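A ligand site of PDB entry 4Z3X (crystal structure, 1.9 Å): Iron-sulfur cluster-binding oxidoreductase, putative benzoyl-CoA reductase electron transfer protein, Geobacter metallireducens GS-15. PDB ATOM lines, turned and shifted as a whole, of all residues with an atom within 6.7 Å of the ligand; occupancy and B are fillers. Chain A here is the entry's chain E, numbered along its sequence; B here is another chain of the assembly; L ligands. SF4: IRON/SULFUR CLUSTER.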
ATOM      1  N   ILE A  15      13.765   3.906  -7.663  1.00  0.00           N
ATOM      2  CA  ILE A  15      12.639   3.456  -8.401  1.00  0.00           C
ATOM      3  C   ILE A  15      12.336   4.459  -9.479  1.00  0.00           C
ATOM      4  O   ILE A  15      11.843   5.556  -9.198  1.00  0.00           O
ATOM      5  CB  ILE A  15      11.412   3.306  -7.514  1.00  0.00           C
ATOM      6  CG1 ILE A  15      11.717   2.470  -6.280  1.00  0.00           C
ATOM      7  CG2 ILE A  15      10.199   2.687  -8.308  1.00  0.00           C
ATOM      8  CD1 ILE A  15      10.570   2.586  -5.152  1.00  0.00           C
ATOM      9  N   LYS A  19      10.189   4.565 -16.055  1.00  0.00           N
ATOM     10  CA  LYS A  19      10.663   3.483 -16.858  1.00  0.00           C
ATOM     11  C   LYS A  19       9.740   2.255 -16.629  1.00  0.00           C
ATOM     12  O   LYS A  19       9.880   1.234 -17.337  1.00  0.00           O
ATOM     13  CB  LYS A  19      12.129   3.164 -16.524  1.00  0.00           C
ATOM     14  CG  LYS A  19      13.204   3.971 -17.207  1.00  0.00           C
ATOM     15  CD  LYS A  19      14.529   3.418 -16.665  1.00  0.00           C
ATOM     16  CE  LYS A  19      15.732   3.745 -17.484  1.00  0.00           C
ATOM     17  NZ  LYS A  19      16.868   2.877 -16.958  1.00  0.00           N
ATOM     18  N   CYS A  20       8.793   2.308 -15.680  1.00  0.00           N
ATOM     19  CA  CYS A  20       8.032   1.092 -15.401  1.00  0.00           C
ATOM     20  C   CYS A  20       6.991   0.821 -16.452  1.00  0.00           C
ATOM     21  O   CYS A  20       6.318   1.761 -16.885  1.00  0.00           O
ATOM     22  CB  CYS A  20       7.333   1.115 -14.052  1.00  0.00           C
ATOM     23  SG  CYS A  20       6.577  -0.478 -13.580  1.00  0.00           S
ATOM     24  N   ASN A  21       6.829  -0.450 -16.829  1.00  0.00           N
ATOM     25  CA  ASN A  21       5.827  -0.817 -17.895  1.00  0.00           C
ATOM     26  C   ASN A  21       4.645  -1.559 -17.311  1.00  0.00           C
ATOM     27  O   ASN A  21       3.804  -2.060 -18.058  1.00  0.00           O
ATOM     28  CB  ASN A  21       6.430  -1.697 -19.024  1.00  0.00           C
ATOM     29  CG  ASN A  21       7.123  -2.930 -18.484  1.00  0.00           C
ATOM     30  OD1 ASN A  21       6.558  -3.650 -17.693  1.00  0.00           O
ATOM     31  ND2 ASN A  21       8.372  -3.147 -18.869  1.00  0.00           N
ATOM     32  N   GLY A  22       4.632  -1.672 -15.979  1.00  0.00           N
ATOM     33  CA  GLY A  22       3.497  -2.265 -15.256  1.00  0.00           C
ATOM     34  C   GLY A  22       3.324  -3.791 -15.313  1.00  0.00           C
ATOM     35  O   GLY A  22       2.207  -4.293 -15.094  1.00  0.00           O
ATOM     36  N   CYS A  23       4.403  -4.516 -15.610  1.00  0.00           N
ATOM     37  CA  CYS A  23       4.344  -5.945 -16.009  1.00  0.00           C
ATOM     38  C   CYS A  23       4.107  -6.793 -14.784  1.00  0.00           C
ATOM     39  O   CYS A  23       3.575  -7.905 -14.867  1.00  0.00           O
ATOM     40  CB  CYS A  23       5.633  -6.383 -16.693  1.00  0.00           C
ATOM     41  SG  CYS A  23       7.099  -6.406 -15.718  1.00  0.00           S
ATOM     42  N   ARG A  24       4.525  -6.253 -13.637  1.00  0.00           N
ATOM     43  CA  ARG A  24       4.382  -6.919 -12.355  1.00  0.00           C
ATOM     44  C   ARG A  24       5.272  -8.133 -12.222  1.00  0.00           C
ATOM     45  O   ARG A  24       5.024  -8.990 -11.379  1.00  0.00           O
ATOM     46  CB  ARG A  24       2.930  -7.286 -12.006  1.00  0.00           C
ATOM     47  CG  ARG A  24       2.025  -6.039 -11.748  1.00  0.00           C
ATOM     48  CD  ARG A  24       0.518  -6.309 -11.794  1.00  0.00           C
ATOM     49  NE  ARG A  24       0.257  -7.405 -10.857  1.00  0.00           N
ATOM     50  CZ  ARG A  24      -0.702  -8.318 -10.952  1.00  0.00           C
ATOM     51  NH1 ARG A  24      -1.590  -8.295 -11.952  1.00  0.00           N
ATOM     52  NH2 ARG A  24      -0.737  -9.268 -10.025  1.00  0.00           N
ATOM     53  N   ALA A  25       6.384  -8.156 -12.954  1.00  0.00           N
ATOM     54  CA  ALA A  25       7.363  -9.283 -12.885  1.00  0.00           C
ATOM     55  C   ALA A  25       8.015  -9.350 -11.489  1.00  0.00           C
ATOM     56  O   ALA A  25       8.402 -10.405 -10.936  1.00  0.00           O
ATOM     57  CB  ALA A  25       8.511  -9.095 -14.057  1.00  0.00           C
ATOM     58  N   CYS A  26       8.171  -8.186 -10.909  1.00  0.00           N
ATOM     59  CA  CYS A  26       8.700  -8.034  -9.568  1.00  0.00           C
ATOM     60  C   CYS A  26       7.844  -8.715  -8.502  1.00  0.00           C
ATOM     61  O   CYS A  26       8.390  -9.436  -7.620  1.00  0.00           O
ATOM     62  CB  CYS A  26       8.875  -6.522  -9.318  1.00  0.00           C
ATOM     63  SG  CYS A  26       7.447  -5.414  -9.737  1.00  0.00           S
ATOM     64  N   GLU A  27       6.528  -8.569  -8.641  1.00  0.00           N
ATOM     65  CA  GLU A  27       5.625  -9.252  -7.726  1.00  0.00           C
ATOM     66  C   GLU A  27       5.729 -10.739  -7.934  1.00  0.00           C
ATOM     67  O   GLU A  27       5.615 -11.472  -6.956  1.00  0.00           O
ATOM     68  CB  GLU A  27       4.173  -8.830  -7.930  1.00  0.00           C
ATOM     69  CG  GLU A  27       3.968  -7.347  -7.893  1.00  0.00           C
ATOM     70  CD  GLU A  27       2.530  -6.910  -7.995  1.00  0.00           C
ATOM     71  OE1 GLU A  27       1.611  -7.737  -8.200  1.00  0.00           O
ATOM     72  OE2 GLU A  27       2.262  -5.710  -7.911  1.00  0.00           O
ATOM     73  N   VAL A  49       6.873  -6.322  -2.774  1.00  0.00           N
ATOM     74  CA  VAL A  49       6.737  -5.151  -3.650  1.00  0.00           C
ATOM     75  C   VAL A  49       5.417  -5.243  -4.386  1.00  0.00           C
ATOM     76  O   VAL A  49       5.085  -6.296  -4.970  1.00  0.00           O
ATOM     77  CB  VAL A  49       7.986  -4.970  -4.654  1.00  0.00           C
ATOM     78  CG1 VAL A  49       8.233  -6.246  -5.520  1.00  0.00           C
ATOM     79  CG2 VAL A  49       7.804  -3.778  -5.629  1.00  0.00           C
ATOM     80  N   VAL A  51       2.768  -3.102  -7.155  1.00  0.00           N
ATOM     81  CA  VAL A  51       2.831  -1.995  -8.129  1.00  0.00           C
ATOM     82  C   VAL A  51       1.506  -1.257  -8.216  1.00  0.00           C
ATOM     83  O   VAL A  51       0.470  -1.851  -8.510  1.00  0.00           O
ATOM     84  CB  VAL A  51       3.217  -2.456  -9.576  1.00  0.00           C
ATOM     85  CG1 VAL A  51       3.309  -1.228 -10.538  1.00  0.00           C
ATOM     86  CG2 VAL A  51       4.548  -3.178  -9.603  1.00  0.00           C
ATOM     87  N   TYR A  60       2.210   4.164 -12.771  1.00  0.00           N
ATOM     88  CA  TYR A  60       2.915   2.852 -12.645  1.00  0.00           C
ATOM     89  C   TYR A  60       3.964   3.160 -11.600  1.00  0.00           C
ATOM     90  O   TYR A  60       5.039   3.770 -11.914  1.00  0.00           O
ATOM     91  CB  TYR A  60       3.554   2.349 -13.977  1.00  0.00           C
ATOM     92  CG  TYR A  60       2.602   2.315 -15.136  1.00  0.00           C
ATOM     93  CD1 TYR A  60       2.319   3.485 -15.811  1.00  0.00           C
ATOM     94  CD2 TYR A  60       1.936   1.133 -15.535  1.00  0.00           C
ATOM     95  CE1 TYR A  60       1.461   3.507 -16.849  1.00  0.00           C
ATOM     96  CE2 TYR A  60       1.062   1.142 -16.627  1.00  0.00           C
ATOM     97  CZ  TYR A  60       0.821   2.352 -17.275  1.00  0.00           C
ATOM     98  OH  TYR A  60      -0.030   2.494 -18.360  1.00  0.00           O
ATOM     99  N   PRO A  62       6.022   1.288  -8.481  1.00  0.00           N
ATOM    100  CA  PRO A  62       6.376   0.155  -7.621  1.00  0.00           C
ATOM    101  C   PRO A  62       6.480   0.633  -6.149  1.00  0.00           C
ATOM    102  O   PRO A  62       7.201   1.574  -5.913  1.00  0.00           O
ATOM    103  CB  PRO A  62       7.767  -0.240  -8.122  1.00  0.00           C
ATOM    104  CG  PRO A  62       7.685   0.211  -9.650  1.00  0.00           C
ATOM    105  CD  PRO A  62       7.069   1.586  -9.462  1.00  0.00           C
ATOM    106  N   TYR A  64       7.382  -0.467  -2.110  1.00  0.00           N
ATOM    107  CA  TYR A  64       8.015  -1.507  -1.292  1.00  0.00           C
ATOM    108  C   TYR A  64       7.448  -1.562   0.094  1.00  0.00           C
ATOM    109  O   TYR A  64       7.171  -0.547   0.648  1.00  0.00           O
ATOM    110  CB  TYR A  64       9.522  -1.280  -1.224  1.00  0.00           C
ATOM    111  CG  TYR A  64      10.191  -1.712  -2.502  1.00  0.00           C
ATOM    112  CD1 TYR A  64       9.997  -1.024  -3.700  1.00  0.00           C
ATOM    113  CD2 TYR A  64      11.052  -2.776  -2.505  1.00  0.00           C
ATOM    114  CE1 TYR A  64      10.582  -1.450  -4.898  1.00  0.00           C
ATOM    115  CE2 TYR A  64      11.644  -3.198  -3.682  1.00  0.00           C
ATOM    116  CZ  TYR A  64      11.417  -2.532  -4.870  1.00  0.00           C
ATOM    117  OH  TYR A  64      12.045  -2.918  -6.066  1.00  0.00           O
ATOM    118  N   CYS A 124      13.661  -8.836  -7.426  1.00  0.00           N
ATOM    119  CA  CYS A 124      12.803  -7.896  -8.186  1.00  0.00           C
ATOM    120  C   CYS A 124      13.692  -7.033  -9.118  1.00  0.00           C
ATOM    121  O   CYS A 124      13.381  -6.890 -10.301  1.00  0.00           O
ATOM    122  CB  CYS A 124      11.982  -7.025  -7.217  1.00  0.00           C
ATOM    123  SG  CYS A 124      13.082  -6.055  -6.022  1.00  0.00           S
ATOM    124  N   TRP A 127      14.788  -9.208 -12.175  1.00  0.00           N
ATOM    125  CA  TRP A 127      13.780  -9.640 -13.142  1.00  0.00           C
ATOM    126  C   TRP A 127      13.185  -8.420 -13.817  1.00  0.00           C
ATOM    127  O   TRP A 127      12.413  -8.580 -14.746  1.00  0.00           O
ATOM    128  CB  TRP A 127      12.646 -10.445 -12.463  1.00  0.00           C
ATOM    129  CG  TRP A 127      12.976 -11.896 -12.413  1.00  0.00           C
ATOM    130  CD1 TRP A 127      14.192 -12.421 -12.122  1.00  0.00           C
ATOM    131  CD2 TRP A 127      12.100 -13.009 -12.707  1.00  0.00           C
ATOM    132  NE1 TRP A 127      14.118 -13.799 -12.171  1.00  0.00           N
ATOM    133  CE2 TRP A 127      12.858 -14.180 -12.552  1.00  0.00           C
ATOM    134  CE3 TRP A 127      10.731 -13.122 -13.041  1.00  0.00           C
ATOM    135  CZ2 TRP A 127      12.320 -15.482 -12.762  1.00  0.00           C
ATOM    136  CZ3 TRP A 127      10.202 -14.412 -13.275  1.00  0.00           C
ATOM    137  CH2 TRP A 127      11.004 -15.577 -13.117  1.00  0.00           C
ATOM    138  N   CYS A 128      13.512  -7.207 -13.331  1.00  0.00           N
ATOM    139  CA  CYS A 128      13.094  -5.975 -14.034  1.00  0.00           C
ATOM    140  C   CYS A 128      14.030  -5.786 -15.227  1.00  0.00           C
ATOM    141  O   CYS A 128      14.987  -4.994 -15.157  1.00  0.00           O
ATOM    142  CB  CYS A 128      13.151  -4.712 -13.128  1.00  0.00           C
ATOM    143  SG  CYS A 128      12.276  -3.302 -13.940  1.00  0.00           S
ATOM    144  N   LEU A 129      13.749  -6.497 -16.322  1.00  0.00           N
ATOM    145  CA  LEU A 129      14.639  -6.448 -17.466  1.00  0.00           C
ATOM    146  C   LEU A 129      14.714  -5.015 -18.029  1.00  0.00           C
ATOM    147  O   LEU A 129      15.720  -4.629 -18.577  1.00  0.00           O
ATOM    148  CB  LEU A 129      14.185  -7.467 -18.561  1.00  0.00           C
ATOM    149  CG  LEU A 129      15.145  -8.686 -18.569  1.00  0.00           C
ATOM    150  CD1 LEU A 129      15.303  -9.334 -17.166  1.00  0.00           C
ATOM    151  CD2 LEU A 129      14.904  -9.789 -19.657  1.00  0.00           C
ATOM    152  N   VAL A 130      13.701  -4.178 -17.811  1.00  0.00           N
ATOM    153  CA  VAL A 130      13.802  -2.810 -18.337  1.00  0.00           C
ATOM    154  C   VAL A 130      14.619  -1.876 -17.372  1.00  0.00           C
ATOM    155  O   VAL A 130      14.938  -0.752 -17.737  1.00  0.00           O
ATOM    156  CB  VAL A 130      12.430  -2.186 -18.647  1.00  0.00           C
ATOM    157  CG1 VAL A 130      11.644  -3.121 -19.675  1.00  0.00           C
ATOM    158  CG2 VAL A 130      11.530  -1.851 -17.295  1.00  0.00           C
ATOM    159  N   GLY A 131      15.008  -2.358 -16.185  1.00  0.00           N
ATOM    160  CA  GLY A 131      15.946  -1.597 -15.358  1.00  0.00           C
ATOM    161  C   GLY A 131      15.327  -0.395 -14.642  1.00  0.00           C
ATOM    162  O   GLY A 131      15.927   0.652 -14.533  1.00  0.00           O
ATOM    163  N   ALA A 132      14.100  -0.544 -14.186  1.00  0.00           N
ATOM    164  CA  ALA A 132      13.369   0.501 -13.464  1.00  0.00           C
ATOM    165  C   ALA A 132      13.861   0.622 -11.986  1.00  0.00           C
ATOM    166  O   ALA A 132      13.547   1.549 -11.290  1.00  0.00           O
ATOM    167  CB  ALA A 132      11.814   0.210 -13.481  1.00  0.00           C
ATOM    168  N   LEU A 133      14.589  -0.383 -11.530  1.00  0.00           N
ATOM    169  CA  LEU A 133      14.829  -0.604 -10.139  1.00  0.00           C
ATOM    170  C   LEU A 133      16.294  -0.862  -9.924  1.00  0.00           C
ATOM    171  O   LEU A 133      16.979  -1.536 -10.716  1.00  0.00           O
ATOM    172  CB  LEU A 133      14.055  -1.778  -9.595  1.00  0.00           C
ATOM    173  CG  LEU A 133      12.607  -1.943  -9.975  1.00  0.00           C
ATOM    174  CD1 LEU A 133      12.254  -3.383  -9.578  1.00  0.00           C
ATOM    175  CD2 LEU A 133      11.698  -0.925  -9.242  1.00  0.00           C
ATOM    176  N   SER B 298       3.468  -3.492 -20.867  1.00  0.00           N
ATOM    177  CA  SER B 298       3.536  -4.916 -21.084  1.00  0.00           C
ATOM    178  C   SER B 298       2.246  -5.674 -20.672  1.00  0.00           C
ATOM    179  O   SER B 298       1.435  -5.181 -19.874  1.00  0.00           O
ATOM    180  CB  SER B 298       4.717  -5.505 -20.307  1.00  0.00           C
ATOM    181  OG  SER B 298       5.996  -5.028 -20.709  1.00  0.00           O
ATOM    182  N   CYS B 302       6.036  -9.766 -18.397  1.00  0.00           N
ATOM    183  CA  CYS B 302       6.825  -9.657 -19.599  1.00  0.00           C
ATOM    184  C   CYS B 302       7.549  -8.322 -19.810  1.00  0.00           C
ATOM    185  O   CYS B 302       6.929  -7.246 -19.669  1.00  0.00           O
ATOM    186  CB  CYS B 302       5.917  -9.911 -20.816  1.00  0.00           C
ATOM    187  SG  CYS B 302       6.810 -10.001 -22.366  1.00  0.00           S
HETATM  188 FE1  SF4 L   1       8.087  -4.267 -11.711  1.00  0.00          FE
HETATM  189 FE2  SF4 L   1       9.979  -3.501 -13.460  1.00  0.00          FE
HETATM  190 FE3  SF4 L   1       7.738  -2.191 -13.148  1.00  0.00          FE
HETATM  191 FE4  SF4 L   1       7.700  -4.576 -14.442  1.00  0.00          FE
HETATM  192  S1  SF4 L   1       8.685  -2.758 -15.249  1.00  0.00           S
HETATM  193  S2  SF4 L   1       6.184  -3.759 -12.813  1.00  0.00           S
HETATM  194  S3  SF4 L   1       9.236  -5.701 -13.187  1.00  0.00           S
HETATM  195  S4  SF4 L   1       9.321  -2.380 -11.505  1.00  0.00           S
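N of Ala 25 lies close to S3 of the ligand. SG of Cys 20 binds FE3 of the ligand (2.1 Å). The backbone NH (N) of Cys 26 sits close to a sulfur (S3) of the ligand (3.5 Å). The side-chain sulfur (SG) of Cys 128 binds an iron atom (FE2) of the ligand (2.4 Å). An iron atom (FE1) of the ligand is bound by the side-chain sulfur of Cys 26 (2.4 Å). S2 of the ligand lies close to N of Cys 23 (3.4 Å). An iron atom (FE4) of the ligand is bound by the side-chain sulfur of Cys 23 (2.3 Å). A sulfur (S1) of the ligand lies close to the side-chain amide oxygen (OD1) of Asn 21 (3.4 Å). N of Asn 21 sits close to S1 of the ligand, at 3.4 Å. N of Arg 24 sits close to S2 of the ligand, 3.1 Å away.
SG of Cys 128 lies close to N of Ala 132, at 3.3 Å. SG of Cys 128 sits close to N of Gly 131 (3.7 Å). The backbone NH of Ser 298 of chain B is in hydrogen-bond range of the backbone carbonyl oxygen of Asn 21, at 3.2 Å. The side-chain carboxylate (OE1) of Glu 27 lies within salt-bridge range of the guanidinium group (NE) of Arg 24, at 3.0 Å. SG of Cys 20 lies close to N of Gly 22 (3.3 Å). OE2 of Glu 27 sits at hydrogen-bond distance from N of Val 51, at 2.8 Å. The backbone NH (N) of Cys 23 lies close to the side-chain amide oxygen (OD1) of Asn 21, 3.1 Å away. The backbone NH (N) of Ala 25 sits close to the side-chain sulfur (SG) of Cys 23, 3.3 Å away.
Residues that only touch the ligand: Pro 62 (3.6 Å), Leu 133 (3.6 Å), Val 130 (3.6 Å), Val 51 (3.6 Å) and Gly 22 (3.8 Å). 12 residues have an atom within 4 Å of the ligand: Cys 20, Asn 21, Gly 22, Cys 23, Arg 24, Ala 25, Cys 26, Val 51, Pro 62, Cys 128, Val 130 and Leu 133. The nearest printed residue that does not touch the ligand is Ala 132 (4.1 Å).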
